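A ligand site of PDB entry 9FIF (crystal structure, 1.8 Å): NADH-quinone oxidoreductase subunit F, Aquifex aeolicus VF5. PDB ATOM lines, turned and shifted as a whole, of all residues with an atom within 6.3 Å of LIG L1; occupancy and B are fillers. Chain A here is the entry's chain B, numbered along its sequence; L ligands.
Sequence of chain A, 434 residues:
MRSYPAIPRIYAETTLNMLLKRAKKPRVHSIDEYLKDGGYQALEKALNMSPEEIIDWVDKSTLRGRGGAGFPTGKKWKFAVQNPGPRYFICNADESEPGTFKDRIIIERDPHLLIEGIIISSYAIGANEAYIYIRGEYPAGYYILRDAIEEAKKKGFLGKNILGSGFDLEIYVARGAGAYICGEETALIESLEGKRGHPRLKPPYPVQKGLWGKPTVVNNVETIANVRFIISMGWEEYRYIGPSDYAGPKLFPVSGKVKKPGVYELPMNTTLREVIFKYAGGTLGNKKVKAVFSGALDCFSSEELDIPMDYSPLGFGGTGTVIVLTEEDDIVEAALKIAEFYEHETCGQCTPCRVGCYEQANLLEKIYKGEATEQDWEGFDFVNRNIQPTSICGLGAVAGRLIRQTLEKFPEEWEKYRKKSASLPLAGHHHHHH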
ATOM      1  N   ILE A 181      27.247 -14.655  18.208  1.00  0.00           N
ATOM      2  CA  ILE A 181      26.710 -15.900  17.693  1.00  0.00           C
ATOM      3  C   ILE A 181      25.283 -16.119  18.181  1.00  0.00           C
ATOM      4  O   ILE A 181      24.534 -16.833  17.537  1.00  0.00           O
ATOM      5  CB  ILE A 181      27.638 -17.092  18.031  1.00  0.00           C
ATOM      6  CG1 ILE A 181      27.276 -18.332  17.239  1.00  0.00           C
ATOM      7  CG2 ILE A 181      27.663 -17.394  19.533  1.00  0.00           C
ATOM      8  CD1 ILE A 181      27.256 -18.094  15.745  1.00  0.00           C
ATOM      9  N   GLY A 197      25.566 -20.251  23.806  1.00  0.00           N
ATOM     10  CA  GLY A 197      25.061 -19.975  22.475  1.00  0.00           C
ATOM     11  C   GLY A 197      25.820 -20.798  21.432  1.00  0.00           C
ATOM     12  O   GLY A 197      26.705 -20.292  20.750  1.00  0.00           O
ATOM     13  N   HIS A 198      25.476 -22.076  21.362  1.00  0.00           N
ATOM     14  CA  HIS A 198      26.068 -22.981  20.413  1.00  0.00           C
ATOM     15  C   HIS A 198      25.045 -23.297  19.332  1.00  0.00           C
ATOM     16  O   HIS A 198      24.054 -23.976  19.599  1.00  0.00           O
ATOM     17  CB  HIS A 198      26.508 -24.274  21.117  1.00  0.00           C
ATOM     18  CG  HIS A 198      27.757 -24.123  21.917  1.00  0.00           C
ATOM     19  ND1 HIS A 198      28.163 -25.120  22.777  1.00  0.00           N
ATOM     20  CD2 HIS A 198      28.720 -23.201  21.949  1.00  0.00           C
ATOM     21  CE1 HIS A 198      29.324 -24.783  23.330  1.00  0.00           C
ATOM     22  NE2 HIS A 198      29.671 -23.611  22.864  1.00  0.00           N
ATOM     23  N   PRO A 199      25.286 -22.893  18.060  1.00  0.00           N
ATOM     24  CA  PRO A 199      24.402 -23.311  16.988  1.00  0.00           C
ATOM     25  C   PRO A 199      24.206 -24.822  16.909  1.00  0.00           C
ATOM     26  O   PRO A 199      25.102 -25.618  17.235  1.00  0.00           O
ATOM     27  CB  PRO A 199      25.058 -22.720  15.736  1.00  0.00           C
ATOM     28  CG  PRO A 199      25.853 -21.547  16.266  1.00  0.00           C
ATOM     29  CD  PRO A 199      26.382 -22.019  17.606  1.00  0.00           C
ATOM     30  N   ARG A 200      22.981 -25.194  16.510  1.00  0.00           N
ATOM     31  CA  ARG A 200      22.605 -26.581  16.319  1.00  0.00           C
ATOM     32  C   ARG A 200      22.756 -26.936  14.841  1.00  0.00           C
ATOM     33  O   ARG A 200      22.535 -26.082  13.981  1.00  0.00           O
ATOM     34  CB  ARG A 200      21.125 -26.805  16.661  1.00  0.00           C
ATOM     35  CG  ARG A 200      20.699 -26.519  18.094  1.00  0.00           C
ATOM     36  CD  ARG A 200      19.159 -26.596  18.235  1.00  0.00           C
ATOM     37  NE  ARG A 200      18.696 -26.256  19.576  1.00  0.00           N
ATOM     38  CZ  ARG A 200      17.418 -26.272  19.981  1.00  0.00           C
ATOM     39  NH1 ARG A 200      16.433 -26.481  19.116  1.00  0.00           N
ATOM     40  NH2 ARG A 200      17.127 -26.077  21.260  1.00  0.00           N
ATOM     41  N   GLU A 345      34.269 -13.980  17.764  1.00  0.00           N
ATOM     42  CA  GLU A 345      32.874 -14.411  17.784  1.00  0.00           C
ATOM     43  C   GLU A 345      32.665 -15.876  17.385  1.00  0.00           C
ATOM     44  O   GLU A 345      31.583 -16.409  17.619  1.00  0.00           O
ATOM     45  CB  GLU A 345      32.029 -13.441  16.947  1.00  0.00           C
ATOM     46  CG  GLU A 345      32.073 -12.001  17.433  1.00  0.00           C
ATOM     47  CD  GLU A 345      31.677 -11.755  18.882  1.00  0.00           C
ATOM     48  OE1 GLU A 345      31.004 -12.616  19.491  1.00  0.00           O
ATOM     49  OE2 GLU A 345      32.099 -10.723  19.443  1.00  0.00           O
ATOM     50  N   THR A 346      33.676 -16.589  16.849  1.00  0.00           N
ATOM     51  CA  THR A 346      33.492 -18.016  16.626  1.00  0.00           C
ATOM     52  C   THR A 346      33.196 -18.674  17.964  1.00  0.00           C
ATOM     53  O   THR A 346      33.826 -18.349  18.962  1.00  0.00           O
ATOM     54  CB  THR A 346      34.701 -18.651  15.937  1.00  0.00           C
ATOM     55  OG1 THR A 346      34.479 -20.071  15.913  1.00  0.00           O
ATOM     56  CG2 THR A 346      36.017 -18.350  16.624  1.00  0.00           C
ATOM     57  N   CYS A 347      32.196 -19.572  17.987  1.00  0.00           N
ATOM     58  CA  CYS A 347      31.831 -20.262  19.212  1.00  0.00           C
ATOM     59  C   CYS A 347      32.742 -21.475  19.475  1.00  0.00           C
ATOM     60  O   CYS A 347      32.703 -22.034  20.554  1.00  0.00           O
ATOM     61  CB  CYS A 347      30.359 -20.685  19.204  1.00  0.00           C
ATOM     62  SG  CYS A 347      29.989 -22.192  18.258  1.00  0.00           S
ATOM     63  N   GLY A 348      33.530 -21.897  18.468  1.00  0.00           N
ATOM     64  CA  GLY A 348      34.555 -22.912  18.657  1.00  0.00           C
ATOM     65  C   GLY A 348      34.101 -24.369  18.505  1.00  0.00           C
ATOM     66  O   GLY A 348      34.928 -25.258  18.639  1.00  0.00           O
ATOM     67  N   GLN A 349      32.837 -24.622  18.154  1.00  0.00           N
ATOM     68  CA  GLN A 349      32.324 -25.981  18.030  1.00  0.00           C
ATOM     69  C   GLN A 349      32.968 -26.743  16.867  1.00  0.00           C
ATOM     70  O   GLN A 349      33.150 -27.969  16.939  1.00  0.00           O
ATOM     71  CB  GLN A 349      30.837 -26.001  17.716  1.00  0.00           C
ATOM     72  CG  GLN A 349      29.937 -25.834  18.930  1.00  0.00           C
ATOM     73  CD  GLN A 349      28.494 -26.037  18.573  1.00  0.00           C
ATOM     74  OE1 GLN A 349      27.841 -25.172  17.959  1.00  0.00           O
ATOM     75  NE2 GLN A 349      28.006 -27.212  18.923  1.00  0.00           N
ATOM     76  N   CYS A 350      33.217 -26.029  15.769  1.00  0.00           N
ATOM     77  CA  CYS A 350      33.686 -26.643  14.550  1.00  0.00           C
ATOM     78  C   CYS A 350      35.172 -26.315  14.411  1.00  0.00           C
ATOM     79  O   CYS A 350      35.564 -25.162  14.581  1.00  0.00           O
ATOM     80  CB  CYS A 350      32.923 -26.134  13.328  1.00  0.00           C
ATOM     81  SG  CYS A 350      31.130 -26.001  13.573  1.00  0.00           S
ATOM     82  N   THR A 351      35.999 -27.309  14.064  1.00  0.00           N
ATOM     83  CA  THR A 351      37.439 -27.129  14.171  1.00  0.00           C
ATOM     84  C   THR A 351      37.944 -26.098  13.156  1.00  0.00           C
ATOM     85  O   THR A 351      38.699 -25.208  13.522  1.00  0.00           O
ATOM     86  CB  THR A 351      38.155 -28.484  14.072  1.00  0.00           C
ATOM     87  OG1 THR A 351      37.957 -29.096  15.342  1.00  0.00           O
ATOM     88  CG2 THR A 351      39.642 -28.341  13.828  1.00  0.00           C
ATOM     89  N   CYS A 353      36.481 -23.613  11.687  1.00  0.00           N
ATOM     90  CA  CYS A 353      36.034 -22.294  12.119  1.00  0.00           C
ATOM     91  C   CYS A 353      36.824 -21.815  13.345  1.00  0.00           C
ATOM     92  O   CYS A 353      37.313 -20.680  13.359  1.00  0.00           O
ATOM     93  CB  CYS A 353      34.545 -22.299  12.409  1.00  0.00           C
ATOM     94  SG  CYS A 353      33.878 -20.699  12.937  1.00  0.00           S
ATOM     95  N   ARG A 354      36.912 -22.673  14.365  1.00  0.00           N
ATOM     96  CA  ARG A 354      37.622 -22.335  15.607  1.00  0.00           C
ATOM     97  C   ARG A 354      39.063 -21.909  15.323  1.00  0.00           C
ATOM     98  O   ARG A 354      39.494 -20.864  15.782  1.00  0.00           O
ATOM     99  CB  ARG A 354      37.645 -23.549  16.544  1.00  0.00           C
ATOM    100  CG  ARG A 354      38.410 -23.349  17.846  1.00  0.00           C
ATOM    101  CD  ARG A 354      38.308 -24.540  18.805  1.00  0.00           C
ATOM    102  NE  ARG A 354      39.043 -25.715  18.318  1.00  0.00           N
ATOM    103  CZ  ARG A 354      38.491 -26.761  17.727  1.00  0.00           C
ATOM    104  NH1 ARG A 354      37.162 -26.826  17.592  1.00  0.00           N
ATOM    105  NH2 ARG A 354      39.267 -27.755  17.306  1.00  0.00           N
ATOM    106  N   CYS A 357      39.340 -18.857  12.254  1.00  0.00           N
ATOM    107  CA  CYS A 357      39.055 -17.473  12.640  1.00  0.00           C
ATOM    108  C   CYS A 357      40.223 -16.929  13.471  1.00  0.00           C
ATOM    109  O   CYS A 357      40.623 -15.768  13.296  1.00  0.00           O
ATOM    110  CB  CYS A 357      37.731 -17.328  13.392  1.00  0.00           C
ATOM    111  SG  CYS A 357      36.259 -17.662  12.387  1.00  0.00           S
ATOM    112  N   ILE A 387      38.132 -21.862   6.347  1.00  0.00           N
ATOM    113  CA  ILE A 387      37.374 -21.670   7.575  1.00  0.00           C
ATOM    114  C   ILE A 387      36.050 -22.427   7.492  1.00  0.00           C
ATOM    115  O   ILE A 387      35.561 -22.933   8.510  1.00  0.00           O
ATOM    116  CB  ILE A 387      37.178 -20.168   7.863  1.00  0.00           C
ATOM    117  CG1 ILE A 387      38.520 -19.406   7.790  1.00  0.00           C
ATOM    118  CG2 ILE A 387      36.460 -19.931   9.196  1.00  0.00           C
ATOM    119  CD1 ILE A 387      38.439 -17.931   8.114  1.00  0.00           C
ATOM    120  N   THR A 390      33.127 -28.169   7.229  1.00  0.00           N
ATOM    121  CA  THR A 390      32.454 -28.826   8.355  1.00  0.00           C
ATOM    122  C   THR A 390      31.655 -27.848   9.223  1.00  0.00           C
ATOM    123  O   THR A 390      31.042 -28.266  10.212  1.00  0.00           O
ATOM    124  CB  THR A 390      33.432 -29.641   9.222  1.00  0.00           C
ATOM    125  OG1 THR A 390      34.135 -28.774  10.109  1.00  0.00           O
ATOM    126  CG2 THR A 390      34.403 -30.468   8.398  1.00  0.00           C
ATOM    127  N   SER A 391      31.611 -26.569   8.859  1.00  0.00           N
ATOM    128  CA  SER A 391      30.889 -25.566   9.638  1.00  0.00           C
ATOM    129  C   SER A 391      29.395 -25.908   9.708  1.00  0.00           C
ATOM    130  O   SER A 391      28.792 -26.343   8.736  1.00  0.00           O
ATOM    131  CB  SER A 391      31.117 -24.196   9.089  1.00  0.00           C
ATOM    132  OG  SER A 391      30.690 -24.096   7.739  1.00  0.00           O
ATOM    133  N   ILE A 392      28.799 -25.719  10.878  1.00  0.00           N
ATOM    134  CA  ILE A 392      27.377 -26.016  11.003  1.00  0.00           C
ATOM    135  C   ILE A 392      26.538 -24.727  11.022  1.00  0.00           C
ATOM    136  O   ILE A 392      25.325 -24.845  11.111  1.00  0.00           O
ATOM    137  CB  ILE A 392      27.108 -26.934  12.209  1.00  0.00           C
ATOM    138  CG1 ILE A 392      27.435 -26.289  13.556  1.00  0.00           C
ATOM    139  CG2 ILE A 392      27.837 -28.256  12.022  1.00  0.00           C
ATOM    140  CD1 ILE A 392      27.251 -27.239  14.730  1.00  0.00           C
ATOM    141  N   CYS A 393      27.148 -23.539  10.972  1.00  0.00           N
ATOM    142  CA  CYS A 393      26.384 -22.298  10.880  1.00  0.00           C
ATOM    143  C   CYS A 393      27.058 -21.340   9.901  1.00  0.00           C
ATOM    144  O   CYS A 393      28.157 -21.580   9.420  1.00  0.00           O
ATOM    145  CB  CYS A 393      26.112 -21.653  12.237  1.00  0.00           C
ATOM    146  SG  CYS A 393      27.337 -20.453  12.842  1.00  0.00           S
ATOM    147  N   GLY A 394      26.370 -20.221   9.625  1.00  0.00           N
ATOM    148  CA  GLY A 394      26.792 -19.254   8.615  1.00  0.00           C
ATOM    149  C   GLY A 394      28.074 -18.502   8.955  1.00  0.00           C
ATOM    150  O   GLY A 394      28.716 -17.996   8.040  1.00  0.00           O
ATOM    151  N   LEU A 395      28.480 -18.434  10.250  1.00  0.00           N
ATOM    152  CA  LEU A 395      29.657 -17.683  10.635  1.00  0.00           C
ATOM    153  C   LEU A 395      30.886 -18.283   9.962  1.00  0.00           C
ATOM    154  O   LEU A 395      31.684 -17.579   9.349  1.00  0.00           O
ATOM    155  CB  LEU A 395      29.829 -17.596  12.159  1.00  0.00           C
ATOM    156  CG  LEU A 395      30.895 -16.610  12.661  1.00  0.00           C
ATOM    157  CD1 LEU A 395      30.567 -16.044  14.022  1.00  0.00           C
ATOM    158  CD2 LEU A 395      32.298 -17.227  12.690  1.00  0.00           C
ATOM    159  N   GLY A 396      31.028 -19.614  10.052  1.00  0.00           N
ATOM    160  CA  GLY A 396      32.170 -20.315   9.483  1.00  0.00           C
ATOM    161  C   GLY A 396      32.181 -20.173   7.966  1.00  0.00           C
ATOM    162  O   GLY A 396      33.238 -19.995   7.352  1.00  0.00           O
ATOM    163  N   ALA A 397      30.986 -20.187   7.381  1.00  0.00           N
ATOM    164  CA  ALA A 397      30.804 -20.056   5.944  1.00  0.00           C
ATOM    165  C   ALA A 397      31.220 -18.672   5.422  1.00  0.00           C
ATOM    166  O   ALA A 397      31.613 -18.583   4.261  1.00  0.00           O
ATOM    167  CB  ALA A 397      29.358 -20.358   5.575  1.00  0.00           C
HETATM  168 FE1  LIG L   1      29.122 -21.587  13.628  1.00  0.00          FE
HETATM  169 FE2  LIG L   1      30.684 -23.820  13.955  1.00  0.00          FE
HETATM  170 FE3  LIG L   1      30.405 -22.068  16.013  1.00  0.00          FE
HETATM  171 FE4  LIG L   1      31.874 -21.380  13.767  1.00  0.00          FE
HETATM  172  S1  LIG L   1      32.381 -22.972  15.312  1.00  0.00           S
HETATM  173  S2  LIG L   1      30.394 -20.063  14.864  1.00  0.00           S
HETATM  174  S3  LIG L   1      30.653 -22.435  12.127  1.00  0.00           S
HETATM  175  S4  LIG L   1      28.741 -23.366  15.036  1.00  0.00           S
HETATM  176  N1  LG2 L   2      19.355 -12.361  12.586  1.00  0.00           N
HETATM  177  C1  LG2 L   2      18.822 -11.310  13.286  1.00  0.00           C
HETATM  178  O1  LG2 L   2      17.622 -11.040  13.237  1.00  0.00           O
HETATM  179  N2  LG2 L   2      19.686 -10.627  14.104  1.00  0.00           N
HETATM  180  C2  LG2 L   2      21.033 -10.912  14.305  1.00  0.00           C
HETATM  181  O2  LG2 L   2      21.675 -10.220  15.097  1.00  0.00           O
HETATM  182  C3  LG2 L   2      21.513 -12.044  13.555  1.00  0.00           C
HETATM  183  N3  LG2 L   2      22.796 -12.460  13.734  1.00  0.00           N
HETATM  184  C4  LG2 L   2      23.260 -13.626  13.094  1.00  0.00           C
HETATM  185  C5  LG2 L   2      24.557 -14.079  13.323  1.00  0.00           C
HETATM  186  C6  LG2 L   2      25.038 -15.216  12.681  1.00  0.00           C
HETATM  187  C7  LG2 L   2      26.457 -15.677  12.938  1.00  0.00           C
HETATM  188  C8  LG2 L   2      24.201 -15.908  11.785  1.00  0.00           C
HETATM  189  C9  LG2 L   2      24.711 -17.070  10.983  1.00  0.00           C
HETATM  190  C10 LG2 L   2      22.898 -15.458  11.568  1.00  0.00           C
HETATM  191  C11 LG2 L   2      22.425 -14.328  12.211  1.00  0.00           C
HETATM  192  N4  LG2 L   2      21.090 -13.853  12.005  1.00  0.00           N
HETATM  193  C12 LG2 L   2      20.670 -12.737  12.703  1.00  0.00           C
HETATM  194  C13 LG2 L   2      20.172 -14.579  11.116  1.00  0.00           C
HETATM  195  C14 LG2 L   2      19.244 -15.486  11.936  1.00  0.00           C
HETATM  196  O3  LG2 L   2      19.864 -16.757  12.144  1.00  0.00           O
HETATM  197  C15 LG2 L   2      17.903 -15.674  11.232  1.00  0.00           C
HETATM  198  O4  LG2 L   2      18.032 -15.988   9.843  1.00  0.00           O
HETATM  199  C16 LG2 L   2      16.915 -14.503  11.372  1.00  0.00           C
HETATM  200  O5  LG2 L   2      16.817 -13.998  12.708  1.00  0.00           O
HETATM  201  C17 LG2 L   2      15.561 -14.922  10.856  1.00  0.00           C
HETATM  202  O6  LG2 L   2      14.625 -13.809  10.852  1.00  0.00           O
HETATM  203  P1  LG2 L   2      14.259 -13.148   9.431  1.00  0.00           P
HETATM  204  O7  LG2 L   2      13.743 -14.265   8.553  1.00  0.00           O
HETATM  205  O8  LG2 L   2      13.183 -12.150   9.834  1.00  0.00           O
HETATM  206  O9  LG2 L   2      15.512 -12.491   8.897  1.00  0.00           O
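Residues that only touch LIG L1: Ile 392 (3.5 Å), Ser 391 (3.5 Å), Pro 199 (3.6 Å), Leu 395 (3.7 Å) and Ile 181 (3.8 Å). Hydrophobic or aromatic side chains that line LIG L1: Ile 181, Pro 199, Ile 392 and Leu 395. The nearest printed residue that does not touch LIG L1 is Arg 354 (4.6 Å).
The side-chain sulfur (SG) of Cys 347 sits close to the side-chain amide oxygen (OE1) of Gln 349. N of Ile 392 lies close to SG of Cys 350 (3.6 Å). O of Cys 353 sits at hydrogen-bond distance from SG of Cys 357 (3.3 Å). N of Cys 353 is in hydrogen-bond range of O of Ile 387, 3.4 Å away. OG1 of Thr 346 lies close to SG of Cys 353. N of Leu 395 lies close to SG of Cys 393. NH1 of Arg 354 is in hydrogen-bond range of O of Gly 348, 2.9 Å away. The backbone NH (N) of Gly 348 lies close to the side-chain hydroxyl (OG1) of Thr 346, 3.3 Å away.
An iron atom (FE2) of LIG L1 is bound by the side-chain sulfur (SG) of Cys 350. The backbone NH (N) of Gly 348 lies close to a sulfur (S1) of LIG L1 (3.5 Å). The side-chain sulfur (SG) of Cys 393 is bound to an iron atom (FE1) of LIG L1. N of Gly 396 sits close to S3 of LIG L1 (3.5 Å). A sulfur (S1) of LIG L1 sits close to the backbone NH (N) of Cys 350 (3.2 Å). A sulfur (S1) of LIG L1 sits close to the side-chain hydroxyl of Thr 346 (3.6 Å). The side-chain amide oxygen (OE1) of Gln 349 lies close to a sulfur (S4) of LIG L1, at 3.6 Å. An iron atom (FE3) of LIG L1 is bound by the side-chain sulfur of Cys 347 (2.3 Å). N of Gln 349 lies close to S1 of LIG L1. The backbone NH (N) of Cys 347 lies close to a sulfur (S2) of LIG L1 (3.6 Å). An iron atom (FE4) of LIG L1 is bound by the side-chain sulfur (SG) of Cys 353, 2.3 Å away.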
